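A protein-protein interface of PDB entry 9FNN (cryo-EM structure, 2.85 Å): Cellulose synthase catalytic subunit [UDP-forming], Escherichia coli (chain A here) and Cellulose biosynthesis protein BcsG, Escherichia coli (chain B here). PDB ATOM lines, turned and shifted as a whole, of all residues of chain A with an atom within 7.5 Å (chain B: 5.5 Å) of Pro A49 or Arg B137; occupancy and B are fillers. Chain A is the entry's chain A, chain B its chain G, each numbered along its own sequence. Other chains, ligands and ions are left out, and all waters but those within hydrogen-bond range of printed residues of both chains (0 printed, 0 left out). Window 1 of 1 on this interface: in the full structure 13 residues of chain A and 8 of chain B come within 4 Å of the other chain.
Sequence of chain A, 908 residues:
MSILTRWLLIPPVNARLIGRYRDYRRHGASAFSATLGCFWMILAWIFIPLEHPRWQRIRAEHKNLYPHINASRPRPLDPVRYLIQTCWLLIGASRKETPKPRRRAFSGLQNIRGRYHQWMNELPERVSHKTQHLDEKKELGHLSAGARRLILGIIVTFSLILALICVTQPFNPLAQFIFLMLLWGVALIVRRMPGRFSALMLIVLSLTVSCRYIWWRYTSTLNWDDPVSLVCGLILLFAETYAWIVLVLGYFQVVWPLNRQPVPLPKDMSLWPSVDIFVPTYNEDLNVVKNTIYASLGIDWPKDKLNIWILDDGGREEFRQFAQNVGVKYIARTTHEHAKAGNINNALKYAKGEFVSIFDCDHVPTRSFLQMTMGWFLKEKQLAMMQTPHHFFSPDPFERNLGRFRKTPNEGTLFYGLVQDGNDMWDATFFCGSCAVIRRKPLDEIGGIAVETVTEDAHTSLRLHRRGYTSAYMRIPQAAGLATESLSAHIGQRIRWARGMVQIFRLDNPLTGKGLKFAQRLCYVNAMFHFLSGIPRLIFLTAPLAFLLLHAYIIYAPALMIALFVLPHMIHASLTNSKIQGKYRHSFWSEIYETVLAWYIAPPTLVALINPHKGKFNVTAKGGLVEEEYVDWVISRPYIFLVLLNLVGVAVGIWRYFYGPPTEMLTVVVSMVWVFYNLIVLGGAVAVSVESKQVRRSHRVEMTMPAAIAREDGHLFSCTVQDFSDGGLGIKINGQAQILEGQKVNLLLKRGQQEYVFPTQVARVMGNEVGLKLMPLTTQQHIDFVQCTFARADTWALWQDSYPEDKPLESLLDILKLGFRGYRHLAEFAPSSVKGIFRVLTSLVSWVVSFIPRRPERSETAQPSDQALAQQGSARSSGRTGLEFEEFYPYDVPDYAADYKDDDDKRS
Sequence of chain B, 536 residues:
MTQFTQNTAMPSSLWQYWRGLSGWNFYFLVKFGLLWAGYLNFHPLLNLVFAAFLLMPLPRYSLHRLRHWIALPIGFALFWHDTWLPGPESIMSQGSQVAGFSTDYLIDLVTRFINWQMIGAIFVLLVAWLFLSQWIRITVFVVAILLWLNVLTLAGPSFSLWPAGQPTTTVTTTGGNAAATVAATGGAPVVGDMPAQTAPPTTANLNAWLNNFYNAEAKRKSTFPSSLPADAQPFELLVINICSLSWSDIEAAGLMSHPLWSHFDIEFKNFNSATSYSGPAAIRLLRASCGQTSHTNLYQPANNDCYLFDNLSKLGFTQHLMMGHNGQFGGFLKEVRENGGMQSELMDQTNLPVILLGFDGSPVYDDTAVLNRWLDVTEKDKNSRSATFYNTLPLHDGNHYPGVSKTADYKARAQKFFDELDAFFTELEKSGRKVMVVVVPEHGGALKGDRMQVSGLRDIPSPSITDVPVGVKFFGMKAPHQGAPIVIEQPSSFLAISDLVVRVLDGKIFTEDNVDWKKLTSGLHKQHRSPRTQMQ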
ATOM      1  N   ILE A  42       6.103  -3.761  17.419  1.00  0.00           N
ATOM      2  CA  ILE A  42       4.812  -4.440  17.389  1.00  0.00           C
ATOM      3  C   ILE A  42       4.713  -5.350  16.172  1.00  0.00           C
ATOM      4  O   ILE A  42       4.247  -6.492  16.274  1.00  0.00           O
ATOM      5  CB  ILE A  42       3.651  -3.426  17.450  1.00  0.00           C
ATOM      6  CG1 ILE A  42       3.707  -2.434  16.288  1.00  0.00           C
ATOM      7  CG2 ILE A  42       3.661  -2.687  18.781  1.00  0.00           C
ATOM      8  CD1 ILE A  42       2.575  -1.432  16.283  1.00  0.00           C
ATOM      9  N   LEU A  43       5.163  -4.877  15.005  1.00  0.00           N
ATOM     10  CA  LEU A  43       5.092  -5.699  13.805  1.00  0.00           C
ATOM     11  C   LEU A  43       5.984  -6.926  13.918  1.00  0.00           C
ATOM     12  O   LEU A  43       5.647  -7.982  13.376  1.00  0.00           O
ATOM     13  CB  LEU A  43       5.466  -4.872  12.576  1.00  0.00           C
ATOM     14  CG  LEU A  43       4.299  -4.244  11.808  1.00  0.00           C
ATOM     15  CD1 LEU A  43       3.422  -5.324  11.196  1.00  0.00           C
ATOM     16  CD2 LEU A  43       3.475  -3.338  12.708  1.00  0.00           C
ATOM     17  N   ALA A  44       7.108  -6.818  14.626  1.00  0.00           N
ATOM     18  CA  ALA A  44       7.937  -7.987  14.883  1.00  0.00           C
ATOM     19  C   ALA A  44       7.229  -8.947  15.826  1.00  0.00           C
ATOM     20  O   ALA A  44       6.985 -10.106  15.480  1.00  0.00           O
ATOM     21  CB  ALA A  44       9.288  -7.558  15.454  1.00  0.00           C
ATOM     22  N   TRP A  45       6.857  -8.469  17.018  1.00  0.00           N
ATOM     23  CA  TRP A  45       6.239  -9.343  18.009  1.00  0.00           C
ATOM     24  C   TRP A  45       5.003 -10.047  17.465  1.00  0.00           C
ATOM     25  O   TRP A  45       4.706 -11.176  17.869  1.00  0.00           O
ATOM     26  CB  TRP A  45       5.891  -8.547  19.268  1.00  0.00           C
ATOM     27  CG  TRP A  45       7.025  -8.448  20.245  1.00  0.00           C
ATOM     28  CD1 TRP A  45       7.976  -7.472  20.304  1.00  0.00           C
ATOM     29  CD2 TRP A  45       7.323  -9.365  21.306  1.00  0.00           C
ATOM     30  NE1 TRP A  45       8.849  -7.723  21.336  1.00  0.00           N
ATOM     31  CE2 TRP A  45       8.470  -8.879  21.967  1.00  0.00           C
ATOM     32  CE3 TRP A  45       6.733 -10.548  21.760  1.00  0.00           C
ATOM     33  CZ2 TRP A  45       9.036  -9.535  23.058  1.00  0.00           C
ATOM     34  CZ3 TRP A  45       7.298 -11.196  22.842  1.00  0.00           C
ATOM     35  CH2 TRP A  45       8.437 -10.691  23.479  1.00  0.00           C
ATOM     36  N   ILE A  46       4.399  -9.488  16.407  1.00  0.00           N
ATOM     37  CA  ILE A  46       3.245 -10.186  15.755  1.00  0.00           C
ATOM     38  C   ILE A  46       3.708 -11.005  14.528  1.00  0.00           C
ATOM     39  O   ILE A  46       3.031 -11.987  14.208  1.00  0.00           O
ATOM     40  CB  ILE A  46       2.092  -9.208  15.422  1.00  0.00           C
ATOM     41  CG1 ILE A  46       2.416  -8.270  14.256  1.00  0.00           C
ATOM     42  CG2 ILE A  46       1.645  -8.451  16.665  1.00  0.00           C
ATOM     43  CD1 ILE A  46       1.341  -7.248  13.973  1.00  0.00           C
ATOM     44  N   PHE A  47       4.812 -10.637  13.867  1.00  0.00           N
ATOM     45  CA  PHE A  47       5.277 -11.359  12.647  1.00  0.00           C
ATOM     46  C   PHE A  47       6.510 -12.203  12.978  1.00  0.00           C
ATOM     47  O   PHE A  47       6.980 -12.900  12.066  1.00  0.00           O
ATOM     48  CB  PHE A  47       5.640 -10.371  11.537  1.00  0.00           C
ATOM     49  CG  PHE A  47       4.482  -9.770  10.779  1.00  0.00           C
ATOM     50  CD1 PHE A  47       3.170 -10.107  11.078  1.00  0.00           C
ATOM     51  CD2 PHE A  47       4.710  -8.883   9.741  1.00  0.00           C
ATOM     52  CE1 PHE A  47       2.115  -9.561  10.364  1.00  0.00           C
ATOM     53  CE2 PHE A  47       3.656  -8.339   9.025  1.00  0.00           C
ATOM     54  CZ  PHE A  47       2.360  -8.676   9.341  1.00  0.00           C
ATOM     55  N   ILE A  48       7.015 -12.134  14.210  1.00  0.00           N
ATOM     56  CA  ILE A  48       8.240 -12.837  14.694  1.00  0.00           C
ATOM     57  C   ILE A  48       7.935 -13.210  16.149  1.00  0.00           C
ATOM     58  O   ILE A  48       7.527 -12.340  16.930  1.00  0.00           O
ATOM     59  CB  ILE A  48       9.491 -11.928  14.626  1.00  0.00           C
ATOM     60  CG1 ILE A  48       9.709 -11.285  13.253  1.00  0.00           C
ATOM     61  CG2 ILE A  48      10.738 -12.661  15.105  1.00  0.00           C
ATOM     62  CD1 ILE A  48      11.026 -10.561  13.114  1.00  0.00           C
ATOM     63  N   PRO A  49       8.073 -14.481  16.553  1.00  0.00           N
ATOM     64  CA  PRO A  49       7.774 -14.931  17.925  1.00  0.00           C
ATOM     65  C   PRO A  49       8.930 -14.654  18.883  1.00  0.00           C
ATOM     66  O   PRO A  49       9.757 -15.508  19.204  1.00  0.00           O
ATOM     67  CB  PRO A  49       7.521 -16.432  17.741  1.00  0.00           C
ATOM     68  CG  PRO A  49       7.737 -16.725  16.263  1.00  0.00           C
ATOM     69  CD  PRO A  49       8.515 -15.596  15.709  1.00  0.00           C
ATOM     70  N   LEU A  50       8.994 -13.409  19.355  1.00  0.00           N
ATOM     71  CA  LEU A  50      10.009 -13.026  20.329  1.00  0.00           C
ATOM     72  C   LEU A  50       9.743 -13.598  21.713  1.00  0.00           C
ATOM     73  O   LEU A  50      10.552 -13.373  22.620  1.00  0.00           O
ATOM     74  CB  LEU A  50      10.120 -11.501  20.415  1.00  0.00           C
ATOM     75  CG  LEU A  50      10.813 -10.755  19.271  1.00  0.00           C
ATOM     76  CD1 LEU A  50      12.046 -11.513  18.792  1.00  0.00           C
ATOM     77  CD2 LEU A  50       9.858 -10.474  18.120  1.00  0.00           C
ATOM     78  N   GLU A  51       8.641 -14.321  21.903  1.00  0.00           N
ATOM     79  CA  GLU A  51       8.372 -14.978  23.174  1.00  0.00           C
ATOM     80  C   GLU A  51       9.153 -16.272  23.349  1.00  0.00           C
ATOM     81  O   GLU A  51       9.094 -16.868  24.429  1.00  0.00           O
ATOM     82  CB  GLU A  51       6.875 -15.264  23.318  1.00  0.00           C
ATOM     83  CG  GLU A  51       6.113 -14.204  24.096  1.00  0.00           C
ATOM     84  CD  GLU A  51       4.613 -14.421  24.059  1.00  0.00           C
ATOM     85  OE1 GLU A  51       4.175 -15.467  23.537  1.00  0.00           O
ATOM     86  OE2 GLU A  51       3.872 -13.541  24.546  1.00  0.00           O
ATOM     87  N   HIS A  52       9.873 -16.718  22.329  1.00  0.00           N
ATOM     88  CA  HIS A  52      10.640 -17.951  22.437  1.00  0.00           C
ATOM     89  C   HIS A  52      11.770 -17.763  23.440  1.00  0.00           C
ATOM     90  O   HIS A  52      12.590 -16.850  23.273  1.00  0.00           O
ATOM     91  CB  HIS A  52      11.193 -18.349  21.071  1.00  0.00           C
ATOM     92  CG  HIS A  52      11.724 -19.749  21.015  1.00  0.00           C
ATOM     93  ND1 HIS A  52      11.911 -20.424  19.827  1.00  0.00           N
ATOM     94  CD2 HIS A  52      12.107 -20.601  21.995  1.00  0.00           C
ATOM     95  CE1 HIS A  52      12.386 -21.630  20.079  1.00  0.00           C
ATOM     96  NE2 HIS A  52      12.515 -21.763  21.387  1.00  0.00           N
ATOM     97  N   PRO A  53      11.850 -18.583  24.490  1.00  0.00           N
ATOM     98  CA  PRO A  53      12.933 -18.420  25.474  1.00  0.00           C
ATOM     99  C   PRO A  53      14.325 -18.595  24.895  1.00  0.00           C
ATOM    100  O   PRO A  53      15.288 -18.108  25.496  1.00  0.00           O
ATOM    101  CB  PRO A  53      12.622 -19.502  26.516  1.00  0.00           C
ATOM    102  CG  PRO A  53      11.150 -19.714  26.402  1.00  0.00           C
ATOM    103  CD  PRO A  53      10.826 -19.539  24.946  1.00  0.00           C
ATOM    104  N   TRP A  55      15.476 -17.217  22.085  1.00  0.00           N
ATOM    105  CA  TRP A  55      15.900 -15.876  21.707  1.00  0.00           C
ATOM    106  C   TRP A  55      16.030 -14.965  22.917  1.00  0.00           C
ATOM    107  O   TRP A  55      16.855 -14.051  22.908  1.00  0.00           O
ATOM    108  CB  TRP A  55      14.929 -15.286  20.689  1.00  0.00           C
ATOM    109  CG  TRP A  55      14.762 -16.171  19.507  1.00  0.00           C
ATOM    110  CD1 TRP A  55      13.613 -16.770  19.090  1.00  0.00           C
ATOM    111  CD2 TRP A  55      15.789 -16.592  18.601  1.00  0.00           C
ATOM    112  NE1 TRP A  55      13.855 -17.525  17.971  1.00  0.00           N
ATOM    113  CE2 TRP A  55      15.184 -17.434  17.650  1.00  0.00           C
ATOM    114  CE3 TRP A  55      17.159 -16.331  18.497  1.00  0.00           C
ATOM    115  CZ2 TRP A  55      15.901 -18.019  16.607  1.00  0.00           C
ATOM    116  CZ3 TRP A  55      17.868 -16.913  17.463  1.00  0.00           C
ATOM    117  CH2 TRP A  55      17.239 -17.749  16.534  1.00  0.00           C
ATOM    118  N   GLN A  56      15.240 -15.198  23.966  1.00  0.00           N
ATOM    119  CA  GLN A  56      15.409 -14.417  25.187  1.00  0.00           C
ATOM    120  C   GLN A  56      16.759 -14.697  25.836  1.00  0.00           C
ATOM    121  O   GLN A  56      17.443 -13.772  26.292  1.00  0.00           O
ATOM    122  CB  GLN A  56      14.266 -14.707  26.157  1.00  0.00           C
ATOM    123  CG  GLN A  56      12.893 -14.591  25.522  1.00  0.00           C
ATOM    124  CD  GLN A  56      12.770 -13.375  24.626  1.00  0.00           C
ATOM    125  OE1 GLN A  56      12.720 -12.240  25.100  1.00  0.00           O
ATOM    126  NE2 GLN A  56      12.726 -13.605  23.319  1.00  0.00           N
ATOM    127  N   TRP B  18      -4.068 -13.386  25.770  1.00  0.00           N
ATOM    128  CA  TRP B  18      -4.005 -13.365  24.311  1.00  0.00           C
ATOM    129  C   TRP B  18      -2.615 -13.870  23.929  1.00  0.00           C
ATOM    130  O   TRP B  18      -1.686 -13.085  23.726  1.00  0.00           O
ATOM    131  CB  TRP B  18      -4.265 -11.962  23.762  1.00  0.00           C
ATOM    132  CG  TRP B  18      -5.678 -11.480  23.924  1.00  0.00           C
ATOM    133  CD1 TRP B  18      -6.298 -11.129  25.086  1.00  0.00           C
ATOM    134  CD2 TRP B  18      -6.637 -11.273  22.879  1.00  0.00           C
ATOM    135  NE1 TRP B  18      -7.588 -10.727  24.833  1.00  0.00           N
ATOM    136  CE2 TRP B  18      -7.820 -10.807  23.485  1.00  0.00           C
ATOM    137  CE3 TRP B  18      -6.612 -11.441  21.492  1.00  0.00           C
ATOM    138  CZ2 TRP B  18      -8.966 -10.507  22.752  1.00  0.00           C
ATOM    139  CZ3 TRP B  18      -7.751 -11.143  20.767  1.00  0.00           C
ATOM    140  CH2 TRP B  18      -8.910 -10.681  21.397  1.00  0.00           C
ATOM    141  N   ARG B  19      -2.479 -15.191  23.831  1.00  0.00           N
ATOM    142  CA  ARG B  19      -1.187 -15.822  23.593  1.00  0.00           C
ATOM    143  C   ARG B  19      -0.907 -16.102  22.125  1.00  0.00           C
ATOM    144  O   ARG B  19       0.260 -16.100  21.720  1.00  0.00           O
ATOM    145  CB  ARG B  19      -1.089 -17.137  24.373  1.00  0.00           C
ATOM    146  CG  ARG B  19      -1.121 -16.971  25.881  1.00  0.00           C
ATOM    147  CD  ARG B  19      -1.298 -18.308  26.581  1.00  0.00           C
ATOM    148  NE  ARG B  19      -2.590 -18.912  26.281  1.00  0.00           N
ATOM    149  CZ  ARG B  19      -3.691 -18.721  26.997  1.00  0.00           C
ATOM    150  NH1 ARG B  19      -3.693 -17.946  28.068  1.00  0.00           N
ATOM    151  NH2 ARG B  19      -4.818 -19.325  26.628  1.00  0.00           N
ATOM    152  N   GLY B  20      -1.935 -16.340  21.325  1.00  0.00           N
ATOM    153  CA  GLY B  20      -1.780 -16.733  19.940  1.00  0.00           C
ATOM    154  C   GLY B  20      -2.357 -18.111  19.697  1.00  0.00           C
ATOM    155  O   GLY B  20      -3.022 -18.701  20.554  1.00  0.00           O
ATOM    156  N   LEU B 132      10.412 -21.917  11.838  1.00  0.00           N
ATOM    157  CA  LEU B 132       9.995 -20.533  11.661  1.00  0.00           C
ATOM    158  C   LEU B 132       9.217 -19.995  12.851  1.00  0.00           C
ATOM    159  O   LEU B 132       8.992 -18.785  12.919  1.00  0.00           O
ATOM    160  CB  LEU B 132       9.160 -20.391  10.387  1.00  0.00           C
ATOM    161  CG  LEU B 132       9.935 -20.488   9.070  1.00  0.00           C
ATOM    162  CD1 LEU B 132       9.012 -20.274   7.880  1.00  0.00           C
ATOM    163  CD2 LEU B 132      11.085 -19.491   9.049  1.00  0.00           C
ATOM    164  N   SER B 133       8.831 -20.849  13.799  1.00  0.00           N
ATOM    165  CA  SER B 133       8.280 -20.379  15.069  1.00  0.00           C
ATOM    166  C   SER B 133       9.325 -19.680  15.924  1.00  0.00           C
ATOM    167  O   SER B 133       9.088 -19.342  17.092  1.00  0.00           O
ATOM    168  CB  SER B 133       7.665 -21.544  15.842  1.00  0.00           C
ATOM    169  OG  SER B 133       8.626 -22.555  16.086  1.00  0.00           O
ATOM    170  N   GLN B 134      10.503 -19.509  15.330  1.00  0.00           N
ATOM    171  CA  GLN B 134      11.582 -18.690  15.857  1.00  0.00           C
ATOM    172  C   GLN B 134      11.581 -17.289  15.258  1.00  0.00           C
ATOM    173  O   GLN B 134      11.690 -16.300  15.989  1.00  0.00           O
ATOM    174  CB  GLN B 134      12.926 -19.372  15.587  1.00  0.00           C
ATOM    175  CG  GLN B 134      13.104 -20.702  16.295  1.00  0.00           C
ATOM    176  CD  GLN B 134      14.307 -21.469  15.784  1.00  0.00           C
ATOM    177  OE1 GLN B 134      14.757 -21.263  14.656  1.00  0.00           O
ATOM    178  NE2 GLN B 134      14.836 -22.359  16.614  1.00  0.00           N
ATOM    179  N   TRP B 135      11.461 -17.187  13.933  1.00  0.00           N
ATOM    180  CA  TRP B 135      11.529 -15.911  13.238  1.00  0.00           C
ATOM    181  C   TRP B 135      10.205 -15.459  12.635  1.00  0.00           C
ATOM    182  O   TRP B 135      10.111 -14.308  12.196  1.00  0.00           O
ATOM    183  CB  TRP B 135      12.584 -15.969  12.122  1.00  0.00           C
ATOM    184  CG  TRP B 135      13.947 -16.365  12.591  1.00  0.00           C
ATOM    185  CD1 TRP B 135      14.450 -17.631  12.673  1.00  0.00           C
ATOM    186  CD2 TRP B 135      14.992 -15.490  13.036  1.00  0.00           C
ATOM    187  NE1 TRP B 135      15.739 -17.600  13.145  1.00  0.00           N
ATOM    188  CE2 TRP B 135      16.096 -16.297  13.375  1.00  0.00           C
ATOM    189  CE3 TRP B 135      15.099 -14.104  13.182  1.00  0.00           C
ATOM    190  CZ2 TRP B 135      17.291 -15.763  13.849  1.00  0.00           C
ATOM    191  CZ3 TRP B 135      16.287 -13.576  13.655  1.00  0.00           C
ATOM    192  CH2 TRP B 135      17.366 -14.405  13.985  1.00  0.00           C
ATOM    193  N   ILE B 136       9.190 -16.321  12.587  1.00  0.00           N
ATOM    194  CA  ILE B 136       7.903 -15.975  11.988  1.00  0.00           C
ATOM    195  C   ILE B 136       6.798 -16.423  12.937  1.00  0.00           C
ATOM    196  O   ILE B 136       6.585 -17.627  13.123  1.00  0.00           O
ATOM    197  CB  ILE B 136       7.708 -16.604  10.601  1.00  0.00           C
ATOM    198  CG1 ILE B 136       8.689 -15.999   9.594  1.00  0.00           C
ATOM    199  CG2 ILE B 136       6.277 -16.407  10.123  1.00  0.00           C
ATOM    200  CD1 ILE B 136       8.472 -14.520   9.344  1.00  0.00           C
ATOM    201  N   ARG B 137       6.092 -15.465  13.532  1.00  0.00           N
ATOM    202  CA  ARG B 137       4.937 -15.781  14.359  1.00  0.00           C
ATOM    203  C   ARG B 137       3.771 -16.122  13.441  1.00  0.00           C
ATOM    204  O   ARG B 137       3.261 -15.255  12.724  1.00  0.00           O
ATOM    205  CB  ARG B 137       4.591 -14.611  15.276  1.00  0.00           C
ATOM    206  CG  ARG B 137       3.708 -14.991  16.456  1.00  0.00           C
ATOM    207  CD  ARG B 137       3.018 -13.773  17.045  1.00  0.00           C
ATOM    208  NE  ARG B 137       2.422 -14.048  18.347  1.00  0.00           N
ATOM    209  CZ  ARG B 137       2.951 -13.673  19.504  1.00  0.00           C
ATOM    210  NH1 ARG B 137       4.083 -12.990  19.560  1.00  0.00           N
ATOM    211  NH2 ARG B 137       2.326 -13.989  20.636  1.00  0.00           N
ATOM    212  N   ILE B 138       3.350 -17.387  13.466  1.00  0.00           N
ATOM    213  CA  ILE B 138       2.407 -17.879  12.469  1.00  0.00           C
ATOM    214  C   ILE B 138       0.978 -17.417  12.730  1.00  0.00           C
ATOM    215  O   ILE B 138       0.171 -17.376  11.793  1.00  0.00           O
ATOM    216  CB  ILE B 138       2.467 -19.414  12.405  1.00  0.00           C
ATOM    217  CG1 ILE B 138       3.913 -19.902  12.523  1.00  0.00           C
ATOM    218  CG2 ILE B 138       1.863 -19.922  11.109  1.00  0.00           C
ATOM    219  CD1 ILE B 138       4.767 -19.584  11.316  1.00  0.00           C
ATOM    220  N   THR B 139       0.643 -17.055  13.971  1.00  0.00           N
ATOM    221  CA  THR B 139      -0.740 -16.716  14.301  1.00  0.00           C
ATOM    222  C   THR B 139      -1.219 -15.491  13.528  1.00  0.00           C
ATOM    223  O   THR B 139      -2.270 -15.524  12.876  1.00  0.00           O
ATOM    224  CB  THR B 139      -0.873 -16.482  15.807  1.00  0.00           C
ATOM    225  OG1 THR B 139      -0.644 -17.712  16.508  1.00  0.00           O
ATOM    226  CG2 THR B 139      -2.260 -15.956  16.146  1.00  0.00           C
ATOM    227  N   VAL B 140      -0.456 -14.399  13.586  1.00  0.00           N
ATOM    228  CA  VAL B 140      -0.891 -13.157  12.955  1.00  0.00           C
ATOM    229  C   VAL B 140      -0.857 -13.280  11.436  1.00  0.00           C
ATOM    230  O   VAL B 140      -1.718 -12.732  10.738  1.00  0.00           O
ATOM    231  CB  VAL B 140      -0.040 -11.979  13.460  1.00  0.00           C
ATOM    232  CG1 VAL B 140      -0.443 -10.685  12.767  1.00  0.00           C
ATOM    233  CG2 VAL B 140      -0.192 -11.846  14.968  1.00  0.00           C
ATOM    234  N   PHE B 141       0.137 -13.990  10.895  1.00  0.00           N
ATOM    235  CA  PHE B 141       0.166 -14.225   9.454  1.00  0.00           C
ATOM    236  C   PHE B 141      -1.044 -15.032   9.001  1.00  0.00           C
ATOM    237  O   PHE B 141      -1.646 -14.734   7.962  1.00  0.00           O
ATOM    238  CB  PHE B 141       1.463 -14.933   9.059  1.00  0.00           C
ATOM    239  CG  PHE B 141       2.600 -13.998   8.765  1.00  0.00           C
ATOM    240  CD1 PHE B 141       2.725 -13.413   7.516  1.00  0.00           C
ATOM    241  CD2 PHE B 141       3.546 -13.706   9.733  1.00  0.00           C
ATOM    242  CE1 PHE B 141       3.769 -12.553   7.237  1.00  0.00           C
ATOM    243  CE2 PHE B 141       4.594 -12.847   9.460  1.00  0.00           C
ATOM    244  CZ  PHE B 141       4.705 -12.269   8.212  1.00  0.00           C
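The backbone carbonyl oxygen (O) of Phe A47 lies within hydrogen-bond range of the backbone NH (N) of Arg B137, at 3.1 Å. The backbone carbonyl oxygen (O) of Trp A45 lies within hydrogen-bond range of the guanidinium group (NH1) of Arg B137 (2.6 Å). The indole nitrogen of Trp A55 lies close to the backbone carbonyl oxygen of Gln B134 (3.2 Å). O of Phe A47 lies close to O of Trp B135. The guanidinium group of Arg B137 is in salt-bridge range of the side-chain carboxylate of Glu A51 (3.7 Å).
O of His A52 sits close to NE2 of Gln A56 (3.2 Å). The backbone carbonyl oxygen (O) of Arg B19 is in hydrogen-bond range of the guanidinium group (NH2) of Arg B137.
Ile A46 touches Val B140. Phe A47 touches Ile B136 (O to CA, 3.2 Å). Phe A47 touches Val B140 (CE1 to CG1, 3.7 Å). CE2 of Phe B141 touches CG of Phe A47, 3.3 Å away. Ile A48 touches Gln B134 (CG2 to O, 3.9 Å). Ile A48 touches Trp B135. Ile A48 touches Arg B137. Pro A49 touches Trp B135 (CD to C, 3.5 Å). Pro A49 touches Arg B137. His A52 touches Gln B134.
Of the printed residues of chain B, Trp A45 touches Arg B137. Of the printed residues of chain B, Ile A48 touches Gln B134 (3.9 Å), Trp B135 (3.2 Å) and Arg B137 (3.5 Å). Printed residues of chain B within 4 Å of His A52: Gln B134 (3.7 Å). Of the printed residues of chain A, Gln B134 touches Ile A48 (3.9 Å), Pro A49 (3.3 Å), His A52 (3.7 Å) and Trp A55 (3.2 Å). Of the printed residues of chain A, Arg B137 touches Trp A45 (2.6 Å), Ile A46 (3.2 Å), Phe A47 (3.1 Å), Ile A48 (3.5 Å), Pro A49 (3.3 Å) and Glu A51 (3.7 Å). Of the printed residues of chain A, Val B140 touches Ile A46 and Phe A47. The nearest printed residue of chain A that does not touch Gln B134 is Leu A50 (5.2 Å).
Printed residues of chain B that touch a printed residue of chain A: Ser B133, Gln B134, Trp B135, Ile B136, Arg B137, Val B140 and Phe B141. Of the 14 printed residues of chain A, 8 touch a printed residue of chain B. Printed residues of chain A that touch a printed residue of chain B: Trp A45, Ile A46, Phe A47, Ile A48, Pro A49, Glu A51, His A52 and Trp A55. Among the printed residues, 20 pairs touch across the chains. Among the printed residues, Asp or Glu carboxylates within 4 Å of a Lys or Arg side-chain nitrogen of the other chain: Glu A51 with Arg B137 (3.7 Å).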
